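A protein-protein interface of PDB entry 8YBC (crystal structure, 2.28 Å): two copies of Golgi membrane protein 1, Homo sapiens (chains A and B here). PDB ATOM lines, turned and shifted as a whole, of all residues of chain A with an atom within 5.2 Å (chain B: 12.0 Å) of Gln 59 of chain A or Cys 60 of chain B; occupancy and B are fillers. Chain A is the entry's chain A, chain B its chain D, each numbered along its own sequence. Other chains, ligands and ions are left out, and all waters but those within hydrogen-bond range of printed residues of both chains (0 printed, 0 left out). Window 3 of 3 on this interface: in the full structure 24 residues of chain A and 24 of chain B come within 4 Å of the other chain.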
ATOM      1  N   GLU A  55      -3.791 -14.009  18.516  1.00  0.00           N
ATOM      2  CA  GLU A  55      -3.409 -15.088  17.615  1.00  0.00           C
ATOM      3  C   GLU A  55      -2.731 -14.538  16.364  1.00  0.00           C
ATOM      4  O   GLU A  55      -1.766 -15.127  15.862  1.00  0.00           O
ATOM      5  CB  GLU A  55      -4.640 -15.919  17.249  1.00  0.00           C
ATOM      6  CG  GLU A  55      -5.457 -16.373  18.456  1.00  0.00           C
ATOM      7  CD  GLU A  55      -6.660 -17.231  18.079  1.00  0.00           C
ATOM      8  OE1 GLU A  55      -6.905 -17.433  16.868  1.00  0.00           O
ATOM      9  OE2 GLU A  55      -7.351 -17.726  18.996  1.00  0.00           O
ATOM     10  N   VAL A  56      -3.223 -13.401  15.855  1.00  0.00           N
ATOM     11  CA  VAL A  56      -2.604 -12.764  14.691  1.00  0.00           C
ATOM     12  C   VAL A  56      -1.131 -12.488  14.957  1.00  0.00           C
ATOM     13  O   VAL A  56      -0.257 -12.885  14.181  1.00  0.00           O
ATOM     14  CB  VAL A  56      -3.352 -11.472  14.324  1.00  0.00           C
ATOM     15  CG1 VAL A  56      -2.444 -10.543  13.522  1.00  0.00           C
ATOM     16  CG2 VAL A  56      -4.615 -11.801  13.535  1.00  0.00           C
ATOM     17  N   LYS A  57      -0.843 -11.804  16.067  1.00  0.00           N
ATOM     18  CA  LYS A  57       0.526 -11.421  16.387  1.00  0.00           C
ATOM     19  C   LYS A  57       1.461 -12.627  16.408  1.00  0.00           C
ATOM     20  O   LYS A  57       2.477 -12.652  15.705  1.00  0.00           O
ATOM     21  CB  LYS A  57       0.539 -10.694  17.727  1.00  0.00           C
ATOM     22  CG  LYS A  57       1.905 -10.258  18.183  1.00  0.00           C
ATOM     23  CD  LYS A  57       1.790  -9.344  19.386  1.00  0.00           C
ATOM     24  CE  LYS A  57       3.052  -8.522  19.579  1.00  0.00           C
ATOM     25  NZ  LYS A  57       3.302  -7.544  18.467  1.00  0.00           N
ATOM     26  N   GLU A  58       1.129 -13.645  17.204  1.00  0.00           N
ATOM     27  CA  GLU A  58       1.971 -14.835  17.295  1.00  0.00           C
ATOM     28  C   GLU A  58       2.242 -15.439  15.921  1.00  0.00           C
ATOM     29  O   GLU A  58       3.388 -15.745  15.574  1.00  0.00           O
ATOM     30  CB  GLU A  58       1.314 -15.867  18.212  1.00  0.00           C
ATOM     31  N   GLN A  59       1.199 -15.606  15.115  1.00  0.00           N
ATOM     32  CA  GLN A  59       1.378 -16.271  13.829  1.00  0.00           C
ATOM     33  C   GLN A  59       2.176 -15.412  12.846  1.00  0.00           C
ATOM     34  O   GLN A  59       3.062 -15.923  12.147  1.00  0.00           O
ATOM     35  CB  GLN A  59       0.020 -16.641  13.256  1.00  0.00           C
ATOM     36  CG  GLN A  59       0.091 -17.249  11.886  1.00  0.00           C
ATOM     37  CD  GLN A  59      -1.140 -18.061  11.567  1.00  0.00           C
ATOM     38  OE1 GLN A  59      -1.773 -17.859  10.537  1.00  0.00           O
ATOM     39  NE2 GLN A  59      -1.487 -18.993  12.451  1.00  0.00           N
ATOM     40  N   CYS A  60       1.889 -14.108  12.775  1.00  0.00           N
ATOM     41  CA  CYS A  60       2.667 -13.264  11.871  1.00  0.00           C
ATOM     42  C   CYS A  60       4.128 -13.183  12.309  1.00  0.00           C
ATOM     43  O   CYS A  60       5.031 -13.233  11.467  1.00  0.00           O
ATOM     44  CB  CYS A  60       2.046 -11.872  11.764  1.00  0.00           C
ATOM     45  SG  CYS A  60       0.442 -11.871  10.876  1.00  0.00           S
ATOM     46  N   GLU A  61       4.384 -13.085  13.622  1.00  0.00           N
ATOM     47  CA  GLU A  61       5.757 -13.156  14.111  1.00  0.00           C
ATOM     48  C   GLU A  61       6.416 -14.468  13.716  1.00  0.00           C
ATOM     49  O   GLU A  61       7.609 -14.486  13.401  1.00  0.00           O
ATOM     50  CB  GLU A  61       5.801 -12.973  15.632  1.00  0.00           C
ATOM     51  CG  GLU A  61       5.395 -11.556  16.085  1.00  0.00           C
ATOM     52  CD  GLU A  61       5.748 -11.230  17.541  1.00  0.00           C
ATOM     53  OE1 GLU A  61       6.120 -10.059  17.809  1.00  0.00           O
ATOM     54  OE2 GLU A  61       5.651 -12.132  18.409  1.00  0.00           O
ATOM     55  N   GLU A  62       5.671 -15.577  13.711  1.00  0.00           N
ATOM     56  CA  GLU A  62       6.265 -16.833  13.264  1.00  0.00           C
ATOM     57  C   GLU A  62       6.653 -16.750  11.801  1.00  0.00           C
ATOM     58  O   GLU A  62       7.707 -17.254  11.396  1.00  0.00           O
ATOM     59  CB  GLU A  62       5.314 -18.004  13.496  1.00  0.00           C
ATOM     60  CG  GLU A  62       5.604 -18.773  14.776  1.00  0.00           C
ATOM     61  CD  GLU A  62       4.812 -20.063  14.875  1.00  0.00           C
ATOM     62  OE1 GLU A  62       4.303 -20.541  13.836  1.00  0.00           O
ATOM     63  OE2 GLU A  62       4.675 -20.581  16.005  1.00  0.00           O
ATOM     64  N   ARG A  63       5.826 -16.099  10.996  1.00  0.00           N
ATOM     65  CA  ARG A  63       6.124 -15.934   9.586  1.00  0.00           C
ATOM     66  C   ARG A  63       7.439 -15.173   9.406  1.00  0.00           C
ATOM     67  O   ARG A  63       7.463 -14.072   8.851  1.00  0.00           O
ATOM     68  CB  ARG A  63       4.956 -15.224   8.908  1.00  0.00           C
ATOM     69  CG  ARG A  63       4.992 -15.242   7.413  1.00  0.00           C
ATOM     70  CD  ARG A  63       4.958 -16.635   6.831  1.00  0.00           C
ATOM     71  NE  ARG A  63       5.432 -16.586   5.450  1.00  0.00           N
ATOM     72  CZ  ARG A  63       4.703 -16.154   4.422  1.00  0.00           C
ATOM     73  NH1 ARG A  63       3.447 -15.756   4.611  1.00  0.00           N
ATOM     74  NH2 ARG A  63       5.222 -16.131   3.197  1.00  0.00           N
ATOM     75  N   ASN B  51     -13.521  -9.584  11.749  1.00  0.00           N
ATOM     76  CA  ASN B  51     -13.342 -10.109  10.394  1.00  0.00           C
ATOM     77  C   ASN B  51     -11.998  -9.700   9.798  1.00  0.00           C
ATOM     78  O   ASN B  51     -11.393 -10.475   9.049  1.00  0.00           O
ATOM     79  CB  ASN B  51     -14.481  -9.655   9.482  1.00  0.00           C
ATOM     80  CG  ASN B  51     -15.842 -10.238   9.893  1.00  0.00           C
ATOM     81  OD1 ASN B  51     -15.934 -11.149  10.735  1.00  0.00           O
ATOM     82  ND2 ASN B  51     -16.903  -9.717   9.286  1.00  0.00           N
ATOM     83  N   GLN B  52     -11.510  -8.501  10.121  1.00  0.00           N
ATOM     84  CA  GLN B  52     -10.167  -8.136   9.702  1.00  0.00           C
ATOM     85  C   GLN B  52      -9.141  -9.089  10.304  1.00  0.00           C
ATOM     86  O   GLN B  52      -8.229  -9.559   9.610  1.00  0.00           O
ATOM     87  CB  GLN B  52      -9.859  -6.690  10.097  1.00  0.00           C
ATOM     88  CG  GLN B  52      -8.775  -6.060   9.246  1.00  0.00           C
ATOM     89  CD  GLN B  52      -7.911  -5.023   9.965  1.00  0.00           C
ATOM     90  OE1 GLN B  52      -6.712  -4.919   9.692  1.00  0.00           O
ATOM     91  NE2 GLN B  52      -8.508  -4.226  10.824  1.00  0.00           N
ATOM     92  N   MET B  53      -9.274  -9.391  11.593  1.00  0.00           N
ATOM     93  CA  MET B  53      -8.278 -10.236  12.239  1.00  0.00           C
ATOM     94  C   MET B  53      -8.321 -11.663  11.698  1.00  0.00           C
ATOM     95  O   MET B  53      -7.279 -12.322  11.609  1.00  0.00           O
ATOM     96  CB  MET B  53      -8.465 -10.174  13.761  1.00  0.00           C
ATOM     97  CG  MET B  53      -8.116  -8.786  14.351  1.00  0.00           C
ATOM     98  SD  MET B  53      -6.372  -8.270  14.168  1.00  0.00           S
ATOM     99  CE  MET B  53      -6.339  -7.362  12.602  1.00  0.00           C
ATOM    100  N   LYS B  54      -9.493 -12.135  11.282  1.00  0.00           N
ATOM    101  CA  LYS B  54      -9.566 -13.410  10.575  1.00  0.00           C
ATOM    102  C   LYS B  54      -8.784 -13.358   9.266  1.00  0.00           C
ATOM    103  O   LYS B  54      -8.114 -14.325   8.888  1.00  0.00           O
ATOM    104  CB  LYS B  54     -11.025 -13.771  10.305  1.00  0.00           C
ATOM    105  CG  LYS B  54     -11.632 -14.754  11.296  1.00  0.00           C
ATOM    106  CD  LYS B  54     -13.075 -14.375  11.628  1.00  0.00           C
ATOM    107  CE  LYS B  54     -13.755 -15.437  12.460  1.00  0.00           C
ATOM    108  NZ  LYS B  54     -15.247 -15.371  12.318  1.00  0.00           N
ATOM    109  N   GLU B  55      -8.872 -12.235   8.550  1.00  0.00           N
ATOM    110  CA  GLU B  55      -8.187 -12.124   7.266  1.00  0.00           C
ATOM    111  C   GLU B  55      -6.667 -12.094   7.438  1.00  0.00           C
ATOM    112  O   GLU B  55      -5.937 -12.728   6.665  1.00  0.00           O
ATOM    113  CB  GLU B  55      -8.681 -10.884   6.531  1.00  0.00           C
ATOM    114  CG  GLU B  55      -7.974 -10.587   5.241  1.00  0.00           C
ATOM    115  CD  GLU B  55      -8.701  -9.519   4.446  1.00  0.00           C
ATOM    116  OE1 GLU B  55      -9.895  -9.709   4.144  1.00  0.00           O
ATOM    117  OE2 GLU B  55      -8.103  -8.465   4.172  1.00  0.00           O
ATOM    118  N   VAL B  56      -6.169 -11.383   8.459  1.00  0.00           N
ATOM    119  CA  VAL B  56      -4.724 -11.328   8.693  1.00  0.00           C
ATOM    120  C   VAL B  56      -4.174 -12.706   9.025  1.00  0.00           C
ATOM    121  O   VAL B  56      -3.062 -13.060   8.608  1.00  0.00           O
ATOM    122  CB  VAL B  56      -4.378 -10.318   9.803  1.00  0.00           C
ATOM    123  CG1 VAL B  56      -2.871 -10.293  10.040  1.00  0.00           C
ATOM    124  CG2 VAL B  56      -4.828  -8.954   9.410  1.00  0.00           C
ATOM    125  N   LYS B  57      -4.922 -13.496   9.798  1.00  0.00           N
ATOM    126  CA  LYS B  57      -4.446 -14.825  10.164  1.00  0.00           C
ATOM    127  C   LYS B  57      -4.167 -15.661   8.921  1.00  0.00           C
ATOM    128  O   LYS B  57      -3.105 -16.285   8.808  1.00  0.00           O
ATOM    129  CB  LYS B  57      -5.460 -15.524  11.074  1.00  0.00           C
ATOM    130  CG  LYS B  57      -5.033 -15.572  12.547  1.00  0.00           C
ATOM    131  CD  LYS B  57      -6.040 -16.314  13.443  1.00  0.00           C
ATOM    132  CE  LYS B  57      -6.741 -17.457  12.713  1.00  0.00           C
ATOM    133  NZ  LYS B  57      -7.882 -18.022  13.503  1.00  0.00           N
ATOM    134  N   GLU B  58      -5.095 -15.665   7.959  1.00  0.00           N
ATOM    135  CA  GLU B  58      -4.881 -16.505   6.785  1.00  0.00           C
ATOM    136  C   GLU B  58      -3.816 -15.928   5.857  1.00  0.00           C
ATOM    137  O   GLU B  58      -3.108 -16.693   5.192  1.00  0.00           O
ATOM    138  CB  GLU B  58      -6.205 -16.751   6.048  1.00  0.00           C
ATOM    139  CG  GLU B  58      -6.708 -15.640   5.128  1.00  0.00           C
ATOM    140  CD  GLU B  58      -8.163 -15.867   4.665  1.00  0.00           C
ATOM    141  OE1 GLU B  58      -8.554 -15.323   3.601  1.00  0.00           O
ATOM    142  OE2 GLU B  58      -8.914 -16.592   5.361  1.00  0.00           O
ATOM    143  N   GLN B  59      -3.660 -14.599   5.806  1.00  0.00           N
ATOM    144  CA  GLN B  59      -2.528 -14.031   5.066  1.00  0.00           C
ATOM    145  C   GLN B  59      -1.203 -14.459   5.687  1.00  0.00           C
ATOM    146  O   GLN B  59      -0.215 -14.674   4.978  1.00  0.00           O
ATOM    147  CB  GLN B  59      -2.615 -12.502   5.017  1.00  0.00           C
ATOM    148  CG  GLN B  59      -3.818 -11.963   4.246  1.00  0.00           C
ATOM    149  CD  GLN B  59      -3.997 -10.450   4.395  1.00  0.00           C
ATOM    150  OE1 GLN B  59      -3.732  -9.867   5.454  1.00  0.00           O
ATOM    151  NE2 GLN B  59      -4.450  -9.810   3.324  1.00  0.00           N
ATOM    152  N   CYS B  60      -1.154 -14.577   7.011  1.00  0.00           N
ATOM    153  CA  CYS B  60       0.094 -14.987   7.627  1.00  0.00           C
ATOM    154  C   CYS B  60       0.251 -16.503   7.655  1.00  0.00           C
ATOM    155  O   CYS B  60       1.338 -16.988   7.979  1.00  0.00           O
ATOM    156  CB  CYS B  60       0.209 -14.387   9.030  1.00  0.00           C
ATOM    157  SG  CYS B  60       0.846 -12.660   9.019  1.00  0.00           S
ATOM    158  N   GLU B  61      -0.795 -17.242   7.269  1.00  0.00           N
ATOM    159  CA  GLU B  61      -0.790 -18.697   7.179  1.00  0.00           C
ATOM    160  C   GLU B  61      -0.636 -19.193   5.744  1.00  0.00           C
ATOM    161  O   GLU B  61      -1.148 -20.266   5.411  1.00  0.00           O
ATOM    162  CB  GLU B  61      -2.076 -19.271   7.779  1.00  0.00           C
ATOM    163  CG  GLU B  61      -1.879 -20.488   8.686  1.00  0.00           C
ATOM    164  CD  GLU B  61      -3.048 -20.710   9.654  1.00  0.00           C
ATOM    165  OE1 GLU B  61      -4.192 -20.947   9.187  1.00  0.00           O
ATOM    166  OE2 GLU B  61      -2.821 -20.641  10.885  1.00  0.00           O
ATOM    167  N   GLU B  62       0.033 -18.437   4.880  1.00  0.00           N
ATOM    168  CA  GLU B  62       0.277 -18.908   3.517  1.00  0.00           C
ATOM    169  C   GLU B  62       1.525 -18.267   2.917  1.00  0.00           C
ATOM    170  O   GLU B  62       1.887 -17.140   3.261  1.00  0.00           O
ATOM    171  CB  GLU B  62      -0.938 -18.631   2.628  1.00  0.00           C
ATOM    172  CG  GLU B  62      -0.836 -17.338   1.842  1.00  0.00           C
ATOM    173  CD  GLU B  62      -1.875 -17.213   0.744  1.00  0.00           C
ATOM    174  OE1 GLU B  62      -2.937 -17.872   0.840  1.00  0.00           O
ATOM    175  OE2 GLU B  62      -1.643 -16.423  -0.198  1.00  0.00           O
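O of Lys 57 of chain B sits close to OE1 of Gln 59 of chain A (2.7 Å).
NE2 of Gln 59 of chain A is in hydrogen-bond range of OE2 of Glu 61 of chain B.
The backbone carbonyl oxygen (O) of Glu 62 of chain B is in hydrogen-bond range of the guanidinium group (NH1) of Arg 63 of chain A, 2.5 Å away.
The side-chain sulfur (SG) of Cys 60 of chain A forms a disulfide with the side-chain sulfur (SG) of Cys 60 of chain B.
OE1 of Glu 55 of chain A is in salt-bridge range of NZ of Lys 57 of chain B (3.6 Å).
CG2 of Val 56 of chain A touches O of Met 53 of chain B (3.3 Å).
Val 56 of chain B touches Val 56 of chain A.
CG2 of Val 56 of chain A touches CG of Lys 57 of chain B (3.9 Å).
Cys 60 of chain B touches Gln 59 of chain A.
SG of Cys 60 of chain A touches CG1 of Val 56 of chain B, at 3.8 Å.
Arg 63 of chain A touches Gln 59 of chain B (NH1 to O, 3.8 Å).
Arg 63 of chain A touches Cys 60 of chain B.
Of the printed residues of chain B, Glu 55 of chain A touches Lys 57.
Of chain B, only Met 53 (3.3 Å), Val 56 (3.5 Å) and Lys 57 (3.9 Å) come within 4 Å of Val 56 of chain A.
Lys 57 of chain A touches none of the printed residues of chain B.
No residue of chain B comes within 4 Å of Glu 58 of chain A.
Cys 60 of chain A touches just these residues of chain B: Val 56 and Cys 60.
No residue of chain B comes within 4 Å of Glu 61 of chain A.
Glu 62 of chain A touches none of the printed residues of chain B.
Of chain B, only Gln 59, Cys 60 and Glu 62 come within 4 Å of Arg 63 of chain A.
Of the printed residues of chain A, Met 53 of chain B touches Val 56 (3.3 Å).
Of chain A, only Gln 59 (3.8 Å), Cys 60 (2.1 Å) and Arg 63 (3.8 Å) come within 4 Å of Cys 60 of chain B.
Printed residues of chain A within 4 Å of Glu 62 of chain B: Arg 63.
Of the 12 printed residues of chain B, 7 touch a printed residue of chain A.
Hydrophobic or aromatic side chains of chain B that line the printed part of chain A: Met 53 and Val 56.
Along chain B the printed residues that touch a printed residue of chain A span positions 53 to 62.
Among the printed residues, 12 pairs touch across the chains.
Glu 55 of chain A touches Lys 57 of chain B, but with the chains exchanged Lys 57 of chain A does not touch Glu 55 of chain B (10.4 Å).
Val 56 of chain A touches Lys 57 of chain B, but with the chains exchanged Lys 57 of chain A does not touch Val 56 of chain B (6.5 Å).
Cys 60 of chain A touches Val 56 of chain B, but with the chains exchanged Val 56 of chain A does not touch Cys 60 of chain B (5.3 Å).
Cys 60 of chain B touches its own counterpart, Cys 60 of chain A.
Positions printed for both chains: 55, 56, 57, 58, 59, 60, 61 and 62.
Of the 12 pairs that touch across the chains among the printed residues, 2 have their exchanged pair printed and touching as well.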
